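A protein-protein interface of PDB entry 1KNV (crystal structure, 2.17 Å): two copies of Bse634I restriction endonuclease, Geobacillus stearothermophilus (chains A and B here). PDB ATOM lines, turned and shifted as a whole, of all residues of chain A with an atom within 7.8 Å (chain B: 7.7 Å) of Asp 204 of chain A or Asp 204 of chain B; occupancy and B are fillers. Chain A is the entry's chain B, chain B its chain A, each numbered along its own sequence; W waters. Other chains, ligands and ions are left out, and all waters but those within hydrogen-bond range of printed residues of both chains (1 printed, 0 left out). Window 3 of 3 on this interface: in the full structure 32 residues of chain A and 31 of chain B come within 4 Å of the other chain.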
ATOM      1  N   LYS A 198      20.510   8.567  17.747  1.00  0.00           N
ATOM      2  CA  LYS A 198      21.005   8.635  19.127  1.00  0.00           C
ATOM      3  C   LYS A 198      21.690   7.349  19.595  1.00  0.00           C
ATOM      4  O   LYS A 198      21.259   6.244  19.270  1.00  0.00           O
ATOM      5  CB  LYS A 198      19.862   8.962  20.102  1.00  0.00           C
ATOM      6  CG  LYS A 198      19.068  10.218  19.792  1.00  0.00           C
ATOM      7  CD  LYS A 198      19.922  11.481  19.774  1.00  0.00           C
ATOM      8  CE  LYS A 198      19.059  12.684  19.397  1.00  0.00           C
ATOM      9  NZ  LYS A 198      19.865  13.893  19.163  1.00  0.00           N
ATOM     10  N   SER A 200      21.663   6.102  22.450  1.00  0.00           N
ATOM     11  CA  SER A 200      20.718   5.385  23.290  1.00  0.00           C
ATOM     12  C   SER A 200      19.594   6.349  23.596  1.00  0.00           C
ATOM     13  O   SER A 200      19.673   7.524  23.239  1.00  0.00           O
ATOM     14  CB  SER A 200      21.384   4.949  24.595  1.00  0.00           C
ATOM     15  OG  SER A 200      21.782   6.073  25.361  1.00  0.00           O
ATOM     16  N   LEU A 201      18.554   5.862  24.260  1.00  0.00           N
ATOM     17  CA  LEU A 201      17.431   6.718  24.600  1.00  0.00           C
ATOM     18  C   LEU A 201      17.501   7.214  26.039  1.00  0.00           C
ATOM     19  O   LEU A 201      16.481   7.409  26.710  1.00  0.00           O
ATOM     20  CB  LEU A 201      16.108   6.004  24.317  1.00  0.00           C
ATOM     21  CG  LEU A 201      15.887   5.782  22.813  1.00  0.00           C
ATOM     22  CD1 LEU A 201      14.512   5.196  22.549  1.00  0.00           C
ATOM     23  CD2 LEU A 201      16.054   7.115  22.087  1.00  0.00           C
ATOM     24  N   ARG A 202      18.730   7.415  26.499  1.00  0.00           N
ATOM     25  CA  ARG A 202      18.990   7.952  27.821  1.00  0.00           C
ATOM     26  C   ARG A 202      18.167   9.250  27.854  1.00  0.00           C
ATOM     27  O   ARG A 202      18.104   9.963  26.856  1.00  0.00           O
ATOM     28  CB  ARG A 202      20.479   8.260  27.928  1.00  0.00           C
ATOM     29  CG  ARG A 202      20.971   8.581  29.318  1.00  0.00           C
ATOM     30  CD  ARG A 202      22.472   8.755  29.303  1.00  0.00           C
ATOM     31  NE  ARG A 202      22.868   9.920  28.525  1.00  0.00           N
ATOM     32  CZ  ARG A 202      24.128  10.292  28.340  1.00  0.00           C
ATOM     33  NH1 ARG A 202      25.111   9.581  28.876  1.00  0.00           N
ATOM     34  NH2 ARG A 202      24.405  11.383  27.632  1.00  0.00           N
ATOM     35  N   PRO A 203      17.538   9.580  28.999  1.00  0.00           N
ATOM     36  CA  PRO A 203      16.715  10.786  29.141  1.00  0.00           C
ATOM     37  C   PRO A 203      17.072  11.992  28.281  1.00  0.00           C
ATOM     38  O   PRO A 203      16.240  12.466  27.508  1.00  0.00           O
ATOM     39  CB  PRO A 203      16.814  11.084  30.627  1.00  0.00           C
ATOM     40  CG  PRO A 203      16.797   9.711  31.204  1.00  0.00           C
ATOM     41  CD  PRO A 203      17.794   8.985  30.324  1.00  0.00           C
ATOM     42  N   ASP A 204      18.299  12.487  28.407  1.00  0.00           N
ATOM     43  CA  ASP A 204      18.716  13.648  27.638  1.00  0.00           C
ATOM     44  C   ASP A 204      18.644  13.420  26.132  1.00  0.00           C
ATOM     45  O   ASP A 204      18.267  14.316  25.384  1.00  0.00           O
ATOM     46  CB  ASP A 204      20.132  14.094  28.052  1.00  0.00           C
ATOM     47  CG  ASP A 204      21.218  13.093  27.669  1.00  0.00           C
ATOM     48  OD1 ASP A 204      20.995  11.870  27.818  1.00  0.00           O
ATOM     49  OD2 ASP A 204      22.308  13.541  27.233  1.00  0.00           O
ATOM     50  N   ARG A 205      18.981  12.219  25.686  1.00  0.00           N
ATOM     51  CA  ARG A 205      18.959  11.916  24.263  1.00  0.00           C
ATOM     52  C   ARG A 205      17.556  11.719  23.742  1.00  0.00           C
ATOM     53  O   ARG A 205      17.261  12.019  22.593  1.00  0.00           O
ATOM     54  CB  ARG A 205      19.805  10.677  23.987  1.00  0.00           C
ATOM     55  CG  ARG A 205      21.287  10.944  24.134  1.00  0.00           C
ATOM     56  CD  ARG A 205      22.056   9.656  24.237  1.00  0.00           C
ATOM     57  NE  ARG A 205      23.484   9.899  24.403  1.00  0.00           N
ATOM     58  CZ  ARG A 205      24.347   8.979  24.816  1.00  0.00           C
ATOM     59  NH1 ARG A 205      23.924   7.758  25.104  1.00  0.00           N
ATOM     60  NH2 ARG A 205      25.628   9.283  24.943  1.00  0.00           N
ATOM     61  N   ARG A 206      16.685  11.214  24.593  1.00  0.00           N
ATOM     62  CA  ARG A 206      15.307  11.008  24.196  1.00  0.00           C
ATOM     63  C   ARG A 206      14.644  12.382  24.054  1.00  0.00           C
ATOM     64  O   ARG A 206      13.864  12.622  23.129  1.00  0.00           O
ATOM     65  CB  ARG A 206      14.587  10.193  25.260  1.00  0.00           C
ATOM     66  CG  ARG A 206      13.331   9.545  24.772  1.00  0.00           C
ATOM     67  CD  ARG A 206      12.670   8.799  25.902  1.00  0.00           C
ATOM     68  NE  ARG A 206      12.051   9.736  26.828  1.00  0.00           N
ATOM     69  CZ  ARG A 206      11.549   9.405  28.011  1.00  0.00           C
ATOM     70  NH1 ARG A 206      11.594   8.147  28.429  1.00  0.00           N
ATOM     71  NH2 ARG A 206      10.989  10.339  28.771  1.00  0.00           N
ATOM     72  N   LEU A 207      14.969  13.279  24.980  1.00  0.00           N
ATOM     73  CA  LEU A 207      14.414  14.618  24.974  1.00  0.00           C
ATOM     74  C   LEU A 207      14.882  15.363  23.731  1.00  0.00           C
ATOM     75  O   LEU A 207      14.128  16.148  23.159  1.00  0.00           O
ATOM     76  CB  LEU A 207      14.824  15.380  26.240  1.00  0.00           C
ATOM     77  CG  LEU A 207      14.133  16.731  26.457  1.00  0.00           C
ATOM     78  CD1 LEU A 207      12.639  16.520  26.581  1.00  0.00           C
ATOM     79  CD2 LEU A 207      14.670  17.403  27.706  1.00  0.00           C
ATOM     80  N   GLN A 208      16.117  15.118  23.300  1.00  0.00           N
ATOM     81  CA  GLN A 208      16.627  15.774  22.098  1.00  0.00           C
ATOM     82  C   GLN A 208      15.796  15.388  20.880  1.00  0.00           C
ATOM     83  O   GLN A 208      15.566  16.209  20.001  1.00  0.00           O
ATOM     84  CB  GLN A 208      18.075  15.394  21.852  1.00  0.00           C
ATOM     85  CG  GLN A 208      18.993  15.872  22.931  1.00  0.00           C
ATOM     86  CD  GLN A 208      20.371  15.268  22.811  1.00  0.00           C
ATOM     87  OE1 GLN A 208      21.228  15.488  23.664  1.00  0.00           O
ATOM     88  NE2 GLN A 208      20.598  14.505  21.752  1.00  0.00           N
ATOM     89  N   LEU A 209      15.355  14.136  20.816  1.00  0.00           N
ATOM     90  CA  LEU A 209      14.539  13.700  19.695  1.00  0.00           C
ATOM     91  C   LEU A 209      13.222  14.438  19.752  1.00  0.00           C
ATOM     92  O   LEU A 209      12.772  14.993  18.758  1.00  0.00           O
ATOM     93  CB  LEU A 209      14.268  12.201  19.765  1.00  0.00           C
ATOM     94  CG  LEU A 209      15.483  11.327  19.480  1.00  0.00           C
ATOM     95  CD1 LEU A 209      15.118   9.868  19.629  1.00  0.00           C
ATOM     96  CD2 LEU A 209      15.979  11.618  18.078  1.00  0.00           C
ATOM     97  N   VAL A 210      12.611  14.455  20.931  1.00  0.00           N
ATOM     98  CA  VAL A 210      11.324  15.116  21.114  1.00  0.00           C
ATOM     99  C   VAL A 210      11.351  16.598  20.748  1.00  0.00           C
ATOM    100  O   VAL A 210      10.488  17.080  20.024  1.00  0.00           O
ATOM    101  CB  VAL A 210      10.820  14.955  22.578  1.00  0.00           C
ATOM    102  CG1 VAL A 210       9.609  15.809  22.804  1.00  0.00           C
ATOM    103  CG2 VAL A 210      10.472  13.494  22.859  1.00  0.00           C
ATOM    104  N   LYS B 198      16.990  24.778  37.891  1.00  0.00           N
ATOM    105  CA  LYS B 198      18.134  23.951  37.523  1.00  0.00           C
ATOM    106  C   LYS B 198      19.379  24.442  38.262  1.00  0.00           C
ATOM    107  O   LYS B 198      19.535  25.636  38.491  1.00  0.00           O
ATOM    108  CB  LYS B 198      18.383  24.021  36.010  1.00  0.00           C
ATOM    109  CG  LYS B 198      17.163  23.754  35.155  1.00  0.00           C
ATOM    110  CD  LYS B 198      16.515  22.404  35.452  1.00  0.00           C
ATOM    111  CE  LYS B 198      15.252  22.208  34.595  1.00  0.00           C
ATOM    112  NZ  LYS B 198      14.526  20.946  34.897  1.00  0.00           N
ATOM    113  N   SER B 200      22.274  24.274  37.069  1.00  0.00           N
ATOM    114  CA  SER B 200      23.060  24.916  36.021  1.00  0.00           C
ATOM    115  C   SER B 200      22.342  24.815  34.677  1.00  0.00           C
ATOM    116  O   SER B 200      21.394  24.047  34.535  1.00  0.00           O
ATOM    117  CB  SER B 200      24.422  24.245  35.891  1.00  0.00           C
ATOM    118  OG  SER B 200      24.296  23.001  35.220  1.00  0.00           O
ATOM    119  N   LEU B 201      22.801  25.591  33.696  1.00  0.00           N
ATOM    120  CA  LEU B 201      22.221  25.568  32.363  1.00  0.00           C
ATOM    121  C   LEU B 201      22.998  24.629  31.456  1.00  0.00           C
ATOM    122  O   LEU B 201      23.250  24.923  30.290  1.00  0.00           O
ATOM    123  CB  LEU B 201      22.185  26.970  31.763  1.00  0.00           C
ATOM    124  CG  LEU B 201      21.180  27.886  32.462  1.00  0.00           C
ATOM    125  CD1 LEU B 201      21.027  29.169  31.674  1.00  0.00           C
ATOM    126  CD2 LEU B 201      19.836  27.175  32.582  1.00  0.00           C
ATOM    127  N   ARG B 202      23.391  23.497  32.021  1.00  0.00           N
ATOM    128  CA  ARG B 202      24.095  22.471  31.279  1.00  0.00           C
ATOM    129  C   ARG B 202      23.110  22.089  30.162  1.00  0.00           C
ATOM    130  O   ARG B 202      21.900  22.027  30.392  1.00  0.00           O
ATOM    131  CB  ARG B 202      24.356  21.291  32.211  1.00  0.00           C
ATOM    132  CG  ARG B 202      25.223  20.205  31.630  1.00  0.00           C
ATOM    133  CD  ARG B 202      25.423  19.107  32.651  1.00  0.00           C
ATOM    134  NE  ARG B 202      24.154  18.496  33.028  1.00  0.00           N
ATOM    135  CZ  ARG B 202      24.017  17.602  33.999  1.00  0.00           C
ATOM    136  NH1 ARG B 202      25.073  17.214  34.706  1.00  0.00           N
ATOM    137  NH2 ARG B 202      22.823  17.088  34.259  1.00  0.00           N
ATOM    138  N   PRO B 203      23.613  21.817  28.948  1.00  0.00           N
ATOM    139  CA  PRO B 203      22.763  21.455  27.805  1.00  0.00           C
ATOM    140  C   PRO B 203      21.468  20.697  28.111  1.00  0.00           C
ATOM    141  O   PRO B 203      20.394  21.121  27.701  1.00  0.00           O
ATOM    142  CB  PRO B 203      23.712  20.659  26.918  1.00  0.00           C
ATOM    143  CG  PRO B 203      25.012  21.369  27.132  1.00  0.00           C
ATOM    144  CD  PRO B 203      25.033  21.554  28.640  1.00  0.00           C
ATOM    145  N   ASP B 204      21.561  19.588  28.839  1.00  0.00           N
ATOM    146  CA  ASP B 204      20.371  18.801  29.149  1.00  0.00           C
ATOM    147  C   ASP B 204      19.349  19.558  29.987  1.00  0.00           C
ATOM    148  O   ASP B 204      18.149  19.480  29.727  1.00  0.00           O
ATOM    149  CB  ASP B 204      20.753  17.463  29.824  1.00  0.00           C
ATOM    150  CG  ASP B 204      21.455  17.637  31.172  1.00  0.00           C
ATOM    151  OD1 ASP B 204      22.317  18.535  31.304  1.00  0.00           O
ATOM    152  OD2 ASP B 204      21.159  16.852  32.100  1.00  0.00           O
ATOM    153  N   ARG B 205      19.824  20.303  30.979  1.00  0.00           N
ATOM    154  CA  ARG B 205      18.937  21.061  31.850  1.00  0.00           C
ATOM    155  C   ARG B 205      18.319  22.240  31.120  1.00  0.00           C
ATOM    156  O   ARG B 205      17.168  22.615  31.369  1.00  0.00           O
ATOM    157  CB  ARG B 205      19.708  21.553  33.065  1.00  0.00           C
ATOM    158  CG  ARG B 205      20.022  20.463  34.063  1.00  0.00           C
ATOM    159  CD  ARG B 205      21.095  20.925  35.038  1.00  0.00           C
ATOM    160  NE  ARG B 205      21.406  19.900  36.024  1.00  0.00           N
ATOM    161  CZ  ARG B 205      22.606  19.734  36.566  1.00  0.00           C
ATOM    162  NH1 ARG B 205      23.610  20.528  36.216  1.00  0.00           N
ATOM    163  NH2 ARG B 205      22.802  18.771  37.455  1.00  0.00           N
ATOM    164  N   ARG B 206      19.091  22.827  30.218  1.00  0.00           N
ATOM    165  CA  ARG B 206      18.611  23.957  29.447  1.00  0.00           C
ATOM    166  C   ARG B 206      17.464  23.477  28.548  1.00  0.00           C
ATOM    167  O   ARG B 206      16.426  24.135  28.437  1.00  0.00           O
ATOM    168  CB  ARG B 206      19.748  24.519  28.598  1.00  0.00           C
ATOM    169  CG  ARG B 206      19.626  25.989  28.274  1.00  0.00           C
ATOM    170  CD  ARG B 206      20.713  26.393  27.302  1.00  0.00           C
ATOM    171  NE  ARG B 206      20.497  25.804  25.981  1.00  0.00           N
ATOM    172  CZ  ARG B 206      21.353  25.902  24.966  1.00  0.00           C
ATOM    173  NH1 ARG B 206      22.496  26.558  25.125  1.00  0.00           N
ATOM    174  NH2 ARG B 206      21.049  25.383  23.776  1.00  0.00           N
ATOM    175  N   LEU B 207      17.654  22.322  27.915  1.00  0.00           N
ATOM    176  CA  LEU B 207      16.639  21.750  27.030  1.00  0.00           C
ATOM    177  C   LEU B 207      15.368  21.387  27.799  1.00  0.00           C
ATOM    178  O   LEU B 207      14.264  21.519  27.279  1.00  0.00           O
ATOM    179  CB  LEU B 207      17.189  20.507  26.335  1.00  0.00           C
ATOM    180  CG  LEU B 207      16.315  19.922  25.227  1.00  0.00           C
ATOM    181  CD1 LEU B 207      16.044  20.988  24.176  1.00  0.00           C
ATOM    182  CD2 LEU B 207      17.017  18.725  24.605  1.00  0.00           C
ATOM    183  N   GLN B 208      15.538  20.912  29.033  1.00  0.00           N
ATOM    184  CA  GLN B 208      14.408  20.554  29.887  1.00  0.00           C
ATOM    185  C   GLN B 208      13.550  21.806  30.093  1.00  0.00           C
ATOM    186  O   GLN B 208      12.316  21.728  30.106  1.00  0.00           O
ATOM    187  CB  GLN B 208      14.904  20.050  31.240  1.00  0.00           C
ATOM    188  CG  GLN B 208      15.412  18.646  31.246  1.00  0.00           C
ATOM    189  CD  GLN B 208      16.303  18.378  32.437  1.00  0.00           C
ATOM    190  OE1 GLN B 208      16.201  19.006  33.492  1.00  0.00           O
ATOM    191  NE2 GLN B 208      17.201  17.414  32.276  1.00  0.00           N
ATOM    192  N   LEU B 209      14.198  22.954  30.256  1.00  0.00           N
ATOM    193  CA  LEU B 209      13.445  24.184  30.454  1.00  0.00           C
ATOM    194  C   LEU B 209      12.697  24.511  29.159  1.00  0.00           C
ATOM    195  O   LEU B 209      11.485  24.739  29.199  1.00  0.00           O
ATOM    196  CB  LEU B 209      14.373  25.337  30.853  1.00  0.00           C
ATOM    197  CG  LEU B 209      14.987  25.242  32.248  1.00  0.00           C
ATOM    198  CD1 LEU B 209      15.901  26.427  32.456  1.00  0.00           C
ATOM    199  CD2 LEU B 209      13.875  25.203  33.267  1.00  0.00           C
ATOM    200  N   VAL B 210      13.393  24.474  28.020  1.00  0.00           N
ATOM    201  CA  VAL B 210      12.765  24.753  26.724  1.00  0.00           C
ATOM    202  C   VAL B 210      11.582  23.848  26.414  1.00  0.00           C
ATOM    203  O   VAL B 210      10.557  24.328  25.978  1.00  0.00           O
ATOM    204  CB  VAL B 210      13.750  24.594  25.562  1.00  0.00           C
ATOM    205  CG1 VAL B 210      12.986  24.715  24.241  1.00  0.00           C
ATOM    206  CG2 VAL B 210      14.856  25.672  25.673  1.00  0.00           C
HETATM  207  O   HOH W   1      18.026  16.918  27.491  1.00  0.00           O
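Among the printed residues, merely in contact across the chains: Asp 204 of chain A with Asp 204 of chain B, Leu 207 of chain A with Leu 207 of chain B, Leu 207 of chain A with Gln 208 of chain B and Gln 208 of chain A with Leu 207 of chain B.
Water W1 lies within hydrogen-bond range of O of Asp 204 of chain A (3.4 Å) and O of Asp 204 of chain B (3.4 Å).
The side-chain amino group (NZ) of Lys 198 of chain B sits at hydrogen-bond distance from the side-chain amide oxygen (OE1) of Gln 208 of chain B, at 2.9 Å. The guanidinium group of Arg 202 of chain B lies within salt-bridge range of the side-chain carboxylate of Asp 204 of chain B, 2.5 Å away. NE2 of Gln 208 of chain B lies close to O of Asp 204 of chain B, 3.4 Å away. The side-chain amide nitrogen of Gln 208 of chain A sits close to the side-chain amino group of Lys 198 of chain A (2.8 Å). OD1 of Asp 204 of chain A lies within salt-bridge range of NE of Arg 202 of chain A, 2.8 Å away.
Asp 204 of chain A touches its own counterpart, Asp 204 of chain B. Leu 207 of chain B touches its own counterpart, Leu 207 of chain A. Leu 207 of chain A touches Gln 208 of chain B, and with the chains exchanged Gln 208 of chain A touches Leu 207 of chain B. Positions printed for both chains: 198, 200, 201, 202, 203, 204, 205, 206, 207, 208, 209 and 210. Of the 4 pairs that touch across the chains among the printed residues, 4 have their exchanged pair printed and touching as well.
Asp 204 of chain A touches just one residue of chain B: Asp 204 (3.9 Å). Of the printed residues of chain B, Leu 207 of chain A touches Leu 207 and Gln 208. Of chain A, only Asp 204 (3.9 Å) comes within 4 Å of Asp 204 of chain B. Arg 206 of chain B touches none of the printed residues of chain A. Printed residues of chain A within 4 Å of Leu 207 of chain B: Leu 207 (3.9 Å) and Gln 208 (3.9 Å). Printed residues of chain A within 4 Å of Gln 208 of chain B: Leu 207. The nearest residue of chain B that does not touch Asp 204 of chain A is Leu 207 of chain B (4.6 Å). The nearest printed residue of chain B that does not touch Leu 207 of chain A is Asp 204 of chain B (4.5 Å).
Of the 12 printed residues of chain A, 3 touch a printed residue of chain B. Printed residues of chain B that touch a printed residue of chain A: Asp 204, Leu 207 and Gln 208. Among the printed residues, no Asp or Glu carboxylate lies within 4 Å of a Lys or Arg side-chain nitrogen of the other chain.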
